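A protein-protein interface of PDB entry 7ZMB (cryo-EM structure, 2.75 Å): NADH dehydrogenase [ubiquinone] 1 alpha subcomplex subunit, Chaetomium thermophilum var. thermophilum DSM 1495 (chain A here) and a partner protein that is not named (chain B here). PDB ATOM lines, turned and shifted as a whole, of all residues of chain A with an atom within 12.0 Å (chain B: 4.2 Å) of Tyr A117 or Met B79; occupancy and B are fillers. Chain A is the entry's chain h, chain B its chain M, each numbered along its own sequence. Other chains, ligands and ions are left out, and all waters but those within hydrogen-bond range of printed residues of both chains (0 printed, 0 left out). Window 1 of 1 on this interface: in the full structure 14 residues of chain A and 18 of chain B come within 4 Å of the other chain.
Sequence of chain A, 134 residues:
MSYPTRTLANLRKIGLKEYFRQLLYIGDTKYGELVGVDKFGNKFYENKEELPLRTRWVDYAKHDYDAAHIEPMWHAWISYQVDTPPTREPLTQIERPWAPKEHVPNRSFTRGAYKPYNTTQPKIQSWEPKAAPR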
ATOM      1  N   ARG A 111      26.024  -8.636  -6.976  1.00  0.00           N
ATOM      2  CA  ARG A 111      26.536  -8.742  -5.619  1.00  0.00           C
ATOM      3  C   ARG A 111      25.567  -8.193  -4.584  1.00  0.00           C
ATOM      4  O   ARG A 111      25.795  -8.379  -3.385  1.00  0.00           O
ATOM      5  CB  ARG A 111      27.885  -8.036  -5.503  1.00  0.00           C
ATOM      6  CG  ARG A 111      29.036  -8.871  -6.015  1.00  0.00           C
ATOM      7  CD  ARG A 111      30.240  -8.045  -6.333  1.00  0.00           C
ATOM      8  NE  ARG A 111      31.415  -8.871  -6.594  1.00  0.00           N
ATOM      9  CZ  ARG A 111      32.579  -8.731  -5.969  1.00  0.00           C
ATOM     10  NH1 ARG A 111      33.597  -9.514  -6.272  1.00  0.00           N
ATOM     11  NH2 ARG A 111      32.725  -7.799  -5.045  1.00  0.00           N
ATOM     12  N   GLY A 112      24.489  -7.550  -5.013  1.00  0.00           N
ATOM     13  CA  GLY A 112      23.408  -7.155  -4.149  1.00  0.00           C
ATOM     14  C   GLY A 112      22.378  -8.228  -3.911  1.00  0.00           C
ATOM     15  O   GLY A 112      21.336  -7.965  -3.308  1.00  0.00           O
ATOM     16  N   ALA A 113      22.646  -9.440  -4.382  1.00  0.00           N
ATOM     17  CA  ALA A 113      21.746 -10.558  -4.154  1.00  0.00           C
ATOM     18  C   ALA A 113      21.555 -10.807  -2.666  1.00  0.00           C
ATOM     19  O   ALA A 113      22.500 -10.735  -1.876  1.00  0.00           O
ATOM     20  CB  ALA A 113      22.289 -11.808  -4.836  1.00  0.00           C
ATOM     21  N   TYR A 114      20.299 -11.050  -2.292  1.00  0.00           N
ATOM     22  CA  TYR A 114      19.923 -11.289  -0.877  1.00  0.00           C
ATOM     23  C   TYR A 114      20.655 -12.506  -0.327  1.00  0.00           C
ATOM     24  O   TYR A 114      20.708 -13.561  -0.982  1.00  0.00           O
ATOM     25  CB  TYR A 114      18.405 -11.462  -0.756  1.00  0.00           C
ATOM     26  CG  TYR A 114      17.907 -12.194   0.463  1.00  0.00           C
ATOM     27  CD1 TYR A 114      17.974 -11.622   1.722  1.00  0.00           C
ATOM     28  CD2 TYR A 114      17.332 -13.447   0.349  1.00  0.00           C
ATOM     29  CE1 TYR A 114      17.504 -12.282   2.843  1.00  0.00           C
ATOM     30  CE2 TYR A 114      16.856 -14.122   1.458  1.00  0.00           C
ATOM     31  CZ  TYR A 114      16.939 -13.536   2.708  1.00  0.00           C
ATOM     32  OH  TYR A 114      16.474 -14.195   3.803  1.00  0.00           O
ATOM     33  N   LYS A 115      21.216 -12.341   0.862  1.00  0.00           N
ATOM     34  CA  LYS A 115      21.884 -13.466   1.542  1.00  0.00           C
ATOM     35  C   LYS A 115      21.038 -13.746   2.782  1.00  0.00           C
ATOM     36  O   LYS A 115      20.874 -12.831   3.596  1.00  0.00           O
ATOM     37  CB  LYS A 115      23.312 -13.039   1.886  1.00  0.00           C
ATOM     38  CG  LYS A 115      24.143 -12.460   0.750  1.00  0.00           C
ATOM     39  CD  LYS A 115      24.451 -13.464  -0.333  1.00  0.00           C
ATOM     40  CE  LYS A 115      25.454 -12.961  -1.348  1.00  0.00           C
ATOM     41  NZ  LYS A 115      26.839 -13.063  -0.836  1.00  0.00           N
ATOM     42  N   PRO A 116      20.506 -14.969   2.965  1.00  0.00           N
ATOM     43  CA  PRO A 116      19.707 -15.313   4.148  1.00  0.00           C
ATOM     44  C   PRO A 116      20.545 -15.450   5.427  1.00  0.00           C
ATOM     45  O   PRO A 116      21.743 -15.551   5.311  1.00  0.00           O
ATOM     46  CB  PRO A 116      19.144 -16.680   3.750  1.00  0.00           C
ATOM     47  CG  PRO A 116      20.222 -17.273   2.888  1.00  0.00           C
ATOM     48  CD  PRO A 116      20.664 -16.097   2.049  1.00  0.00           C
ATOM     49  N   TYR A 117      19.923 -15.395   6.603  1.00  0.00           N
ATOM     50  CA  TYR A 117      20.675 -15.632   7.862  1.00  0.00           C
ATOM     51  C   TYR A 117      19.767 -15.965   9.043  1.00  0.00           C
ATOM     52  O   TYR A 117      18.553 -15.759   8.935  1.00  0.00           O
ATOM     53  CB  TYR A 117      21.530 -14.428   8.267  1.00  0.00           C
ATOM     54  CG  TYR A 117      20.849 -13.086   8.264  1.00  0.00           C
ATOM     55  CD1 TYR A 117      20.692 -12.374   7.088  1.00  0.00           C
ATOM     56  CD2 TYR A 117      20.396 -12.512   9.436  1.00  0.00           C
ATOM     57  CE1 TYR A 117      20.068 -11.141   7.071  1.00  0.00           C
ATOM     58  CE2 TYR A 117      19.784 -11.270   9.440  1.00  0.00           C
ATOM     59  CZ  TYR A 117      19.622 -10.583   8.253  1.00  0.00           C
ATOM     60  OH  TYR A 117      19.028  -9.358   8.237  1.00  0.00           O
ATOM     61  N   ASN A 118      20.354 -16.480  10.125  1.00  0.00           N
ATOM     62  CA  ASN A 118      19.625 -16.682  11.363  1.00  0.00           C
ATOM     63  C   ASN A 118      19.359 -15.329  12.019  1.00  0.00           C
ATOM     64  O   ASN A 118      20.287 -14.552  12.240  1.00  0.00           O
ATOM     65  CB  ASN A 118      20.450 -17.584  12.277  1.00  0.00           C
ATOM     66  CG  ASN A 118      19.622 -18.284  13.330  1.00  0.00           C
ATOM     67  OD1 ASN A 118      18.461 -17.960  13.555  1.00  0.00           O
ATOM     68  ND2 ASN A 118      20.233 -19.239  13.996  1.00  0.00           N
ATOM     69  N   THR A 119      18.098 -15.040  12.317  1.00  0.00           N
ATOM     70  CA  THR A 119      17.736 -13.826  13.034  1.00  0.00           C
ATOM     71  C   THR A 119      17.668 -14.033  14.540  1.00  0.00           C
ATOM     72  O   THR A 119      17.320 -13.101  15.264  1.00  0.00           O
ATOM     73  CB  THR A 119      16.388 -13.288  12.535  1.00  0.00           C
ATOM     74  OG1 THR A 119      15.362 -14.257  12.766  1.00  0.00           O
ATOM     75  CG2 THR A 119      16.447 -12.968  11.056  1.00  0.00           C
ATOM     76  N   THR A 120      18.002 -15.223  15.022  1.00  0.00           N
ATOM     77  CA  THR A 120      17.821 -15.597  16.412  1.00  0.00           C
ATOM     78  C   THR A 120      19.175 -15.955  17.014  1.00  0.00           C
ATOM     79  O   THR A 120      20.095 -16.365  16.305  1.00  0.00           O
ATOM     80  CB  THR A 120      16.824 -16.769  16.521  1.00  0.00           C
ATOM     81  OG1 THR A 120      15.566 -16.372  15.968  1.00  0.00           O
ATOM     82  CG2 THR A 120      16.576 -17.161  17.955  1.00  0.00           C
ATOM     83  N   GLN A 121      19.306 -15.757  18.322  1.00  0.00           N
ATOM     84  CA  GLN A 121      20.504 -16.129  19.057  1.00  0.00           C
ATOM     85  C   GLN A 121      20.600 -17.643  19.210  1.00  0.00           C
ATOM     86  O   GLN A 121      19.612 -18.356  19.036  1.00  0.00           O
ATOM     87  CB  GLN A 121      20.502 -15.462  20.431  1.00  0.00           C
ATOM     88  CG  GLN A 121      20.721 -13.956  20.412  1.00  0.00           C
ATOM     89  CD  GLN A 121      22.119 -13.564  20.017  1.00  0.00           C
ATOM     90  OE1 GLN A 121      22.558 -13.813  18.900  1.00  0.00           O
ATOM     91  NE2 GLN A 121      22.828 -12.930  20.931  1.00  0.00           N
ATOM     92  N   PRO A 122      21.788 -18.163  19.509  1.00  0.00           N
ATOM     93  CA  PRO A 122      21.912 -19.600  19.764  1.00  0.00           C
ATOM     94  C   PRO A 122      21.108 -20.025  20.984  1.00  0.00           C
ATOM     95  O   PRO A 122      20.771 -19.215  21.850  1.00  0.00           O
ATOM     96  CB  PRO A 122      23.417 -19.793  19.982  1.00  0.00           C
ATOM     97  CG  PRO A 122      23.926 -18.452  20.322  1.00  0.00           C
ATOM     98  CD  PRO A 122      23.104 -17.509  19.509  1.00  0.00           C
ATOM     99  N   LYS A 123      20.800 -21.318  21.040  1.00  0.00           N
ATOM    100  CA  LYS A 123      19.793 -21.788  21.982  1.00  0.00           C
ATOM    101  C   LYS A 123      20.406 -22.240  23.301  1.00  0.00           C
ATOM    102  O   LYS A 123      19.729 -22.247  24.333  1.00  0.00           O
ATOM    103  CB  LYS A 123      18.973 -22.905  21.341  1.00  0.00           C
ATOM    104  CG  LYS A 123      18.328 -22.470  20.039  1.00  0.00           C
ATOM    105  CD  LYS A 123      16.931 -23.002  19.887  1.00  0.00           C
ATOM    106  CE  LYS A 123      16.473 -22.898  18.444  1.00  0.00           C
ATOM    107  NZ  LYS A 123      16.493 -21.495  17.955  1.00  0.00           N
ATOM    108  N   ALA B  57      25.487  -2.719   7.799  1.00  0.00           N
ATOM    109  CA  ALA B  57      25.807  -4.120   8.098  1.00  0.00           C
ATOM    110  C   ALA B  57      25.991  -4.232   9.606  1.00  0.00           C
ATOM    111  O   ALA B  57      26.195  -5.351  10.095  1.00  0.00           O
ATOM    112  CB  ALA B  57      27.067  -4.469   7.379  1.00  0.00           C
ATOM    113  N   ARG B  75      22.888  -7.585  13.920  1.00  0.00           N
ATOM    114  CA  ARG B  75      23.165  -7.605  12.461  1.00  0.00           C
ATOM    115  C   ARG B  75      24.662  -7.836  12.228  1.00  0.00           C
ATOM    116  O   ARG B  75      24.987  -8.602  11.319  1.00  0.00           O
ATOM    117  CB  ARG B  75      22.605  -6.358  11.763  1.00  0.00           C
ATOM    118  CG  ARG B  75      22.693  -6.421  10.247  1.00  0.00           C
ATOM    119  CD  ARG B  75      22.029  -5.264   9.536  1.00  0.00           C
ATOM    120  NE  ARG B  75      20.577  -5.349   9.558  1.00  0.00           N
ATOM    121  CZ  ARG B  75      19.841  -5.908   8.605  1.00  0.00           C
ATOM    122  NH1 ARG B  75      18.526  -5.929   8.714  1.00  0.00           N
ATOM    123  NH2 ARG B  75      20.423  -6.441   7.546  1.00  0.00           N
ATOM    124  N   GLU B  77      26.604  -9.581  13.913  1.00  0.00           N
ATOM    125  CA  GLU B  77      26.910 -10.983  14.149  1.00  0.00           C
ATOM    126  C   GLU B  77      26.302 -11.904  13.102  1.00  0.00           C
ATOM    127  O   GLU B  77      26.568 -13.107  13.129  1.00  0.00           O
ATOM    128  CB  GLU B  77      26.428 -11.400  15.536  1.00  0.00           C
ATOM    129  CG  GLU B  77      27.091 -10.656  16.666  1.00  0.00           C
ATOM    130  CD  GLU B  77      26.648 -11.159  18.024  1.00  0.00           C
ATOM    131  OE1 GLU B  77      26.089 -12.276  18.096  1.00  0.00           O
ATOM    132  OE2 GLU B  77      26.851 -10.436  19.020  1.00  0.00           O
ATOM    133  N   ALA B  78      25.501 -11.379  12.182  1.00  0.00           N
ATOM    134  CA  ALA B  78      24.893 -12.192  11.145  1.00  0.00           C
ATOM    135  C   ALA B  78      25.291 -11.789   9.735  1.00  0.00           C
ATOM    136  O   ALA B  78      25.090 -12.583   8.813  1.00  0.00           O
ATOM    137  CB  ALA B  78      23.363 -12.158  11.268  1.00  0.00           C
ATOM    138  N   MET B  79      25.845 -10.592   9.540  1.00  0.00           N
ATOM    139  CA  MET B  79      26.464 -10.184   8.285  1.00  0.00           C
ATOM    140  C   MET B  79      27.920 -10.605   8.190  1.00  0.00           C
ATOM    141  O   MET B  79      28.609 -10.185   7.259  1.00  0.00           O
ATOM    142  CB  MET B  79      26.406  -8.661   8.103  1.00  0.00           C
ATOM    143  CG  MET B  79      25.050  -7.996   8.171  1.00  0.00           C
ATOM    144  SD  MET B  79      23.988  -8.274   6.756  1.00  0.00           S
ATOM    145  CE  MET B  79      22.924  -9.503   7.456  1.00  0.00           C
ATOM    146  N   ALA B  80      28.426 -11.371   9.141  1.00  0.00           N
ATOM    147  CA  ALA B  80      29.809 -11.814   9.083  1.00  0.00           C
ATOM    148  C   ALA B  80      29.883 -13.231   8.531  1.00  0.00           C
ATOM    149  O   ALA B  80      28.904 -13.976   8.530  1.00  0.00           O
ATOM    150  CB  ALA B  80      30.459 -11.747  10.463  1.00  0.00           C
ATOM    151  N   ARG B  83      29.907 -16.037   3.623  1.00  0.00           N
ATOM    152  CA  ARG B  83      28.738 -15.777   2.751  1.00  0.00           C
ATOM    153  C   ARG B  83      28.557 -14.271   2.548  1.00  0.00           C
ATOM    154  O   ARG B  83      27.688 -13.889   1.760  1.00  0.00           O
ATOM    155  CB  ARG B  83      27.512 -16.417   3.398  1.00  0.00           C
ATOM    156  CG  ARG B  83      27.534 -17.938   3.385  1.00  0.00           C
ATOM    157  CD  ARG B  83      26.168 -18.533   3.650  1.00  0.00           C
ATOM    158  NE  ARG B  83      25.568 -17.980   4.856  1.00  0.00           N
ATOM    159  CZ  ARG B  83      24.509 -17.179   4.885  1.00  0.00           C
ATOM    160  NH1 ARG B  83      24.057 -16.737   6.045  1.00  0.00           N
ATOM    161  NH2 ARG B  83      23.897 -16.838   3.766  1.00  0.00           N
ATOM    162  N   PHE B  84      29.354 -13.452   3.231  1.00  0.00           N
ATOM    163  CA  PHE B  84      29.204 -11.977   3.160  1.00  0.00           C
ATOM    164  C   PHE B  84      30.497 -11.320   2.667  1.00  0.00           C
ATOM    165  O   PHE B  84      30.754 -10.184   3.091  1.00  0.00           O
ATOM    166  CB  PHE B  84      28.714 -11.515   4.533  1.00  0.00           C
ATOM    167  CG  PHE B  84      27.312 -11.955   4.868  1.00  0.00           C
ATOM    168  CD1 PHE B  84      26.221 -11.196   4.474  1.00  0.00           C
ATOM    169  CD2 PHE B  84      27.081 -13.131   5.563  1.00  0.00           C
ATOM    170  CE1 PHE B  84      24.932 -11.602   4.773  1.00  0.00           C
ATOM    171  CE2 PHE B  84      25.790 -13.538   5.855  1.00  0.00           C
ATOM    172  CZ  PHE B  84      24.718 -12.771   5.463  1.00  0.00           C
ATOM    173  N   PHE B  89      26.105  -4.398   1.067  1.00  0.00           N
ATOM    174  CA  PHE B  89      25.360  -4.369   2.350  1.00  0.00           C
ATOM    175  C   PHE B  89      24.085  -3.541   2.286  1.00  0.00           C
ATOM    176  O   PHE B  89      23.128  -3.884   2.976  1.00  0.00           O
ATOM    177  CB  PHE B  89      26.304  -4.086   3.515  1.00  0.00           C
ATOM    178  CG  PHE B  89      27.144  -5.273   3.911  1.00  0.00           C
ATOM    179  CD1 PHE B  89      26.556  -6.406   4.448  1.00  0.00           C
ATOM    180  CD2 PHE B  89      28.517  -5.265   3.739  1.00  0.00           C
ATOM    181  CE1 PHE B  89      27.323  -7.501   4.809  1.00  0.00           C
ATOM    182  CE2 PHE B  89      29.282  -6.362   4.097  1.00  0.00           C
ATOM    183  CZ  PHE B  89      28.684  -7.477   4.632  1.00  0.00           C
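O of Pro A116 lies within hydrogen-bond range of NH1 of Arg B83, 2.7 Å away. O of Arg B83 is in hydrogen-bond range of NZ of Lys A115 (2.9 Å). NH2 of Arg B75 lies within hydrogen-bond range of OH of Tyr A117.
Among the printed residues, merely in contact across the chains: Lys A115 with Phe B84, Tyr A117 with Ala B78, Tyr A117 with Met B79, Tyr A117 with Arg B83 and Gln A121 with Glu B77.
Arg A111 touches none of the printed residues of chain B. Of the printed residues of chain B, Tyr A117 touches Arg B75, Ala B78, Met B79 and Arg B83. Arg B75 touches just one residue of chain A: Tyr A117. Printed residues of chain A within 4 Å of Glu B77: Gln A121 (3.9 Å). Of the printed residues of chain A, Ala B78 touches Tyr A117. Of the printed residues of chain A, Met B79 touches Tyr A117. No residue of chain A comes within 4 Å of Ala B80. The nearest residue of chain A that does not touch Met B79 is Lys A115 (5.5 Å). The nearest printed residue of chain B that does not touch Pro A116 is Phe B84 (4.1 Å).
Of the 9 printed residues of chain B, 6 touch a printed residue of chain A. Of the 13 printed residues of chain A, 4 touch a printed residue of chain B. Hydrophobic or aromatic side chains of chain A within 4 Å of the printed part of chain B: Pro A116 and Tyr A117. Among the printed residues, 8 pairs touch across the chains.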
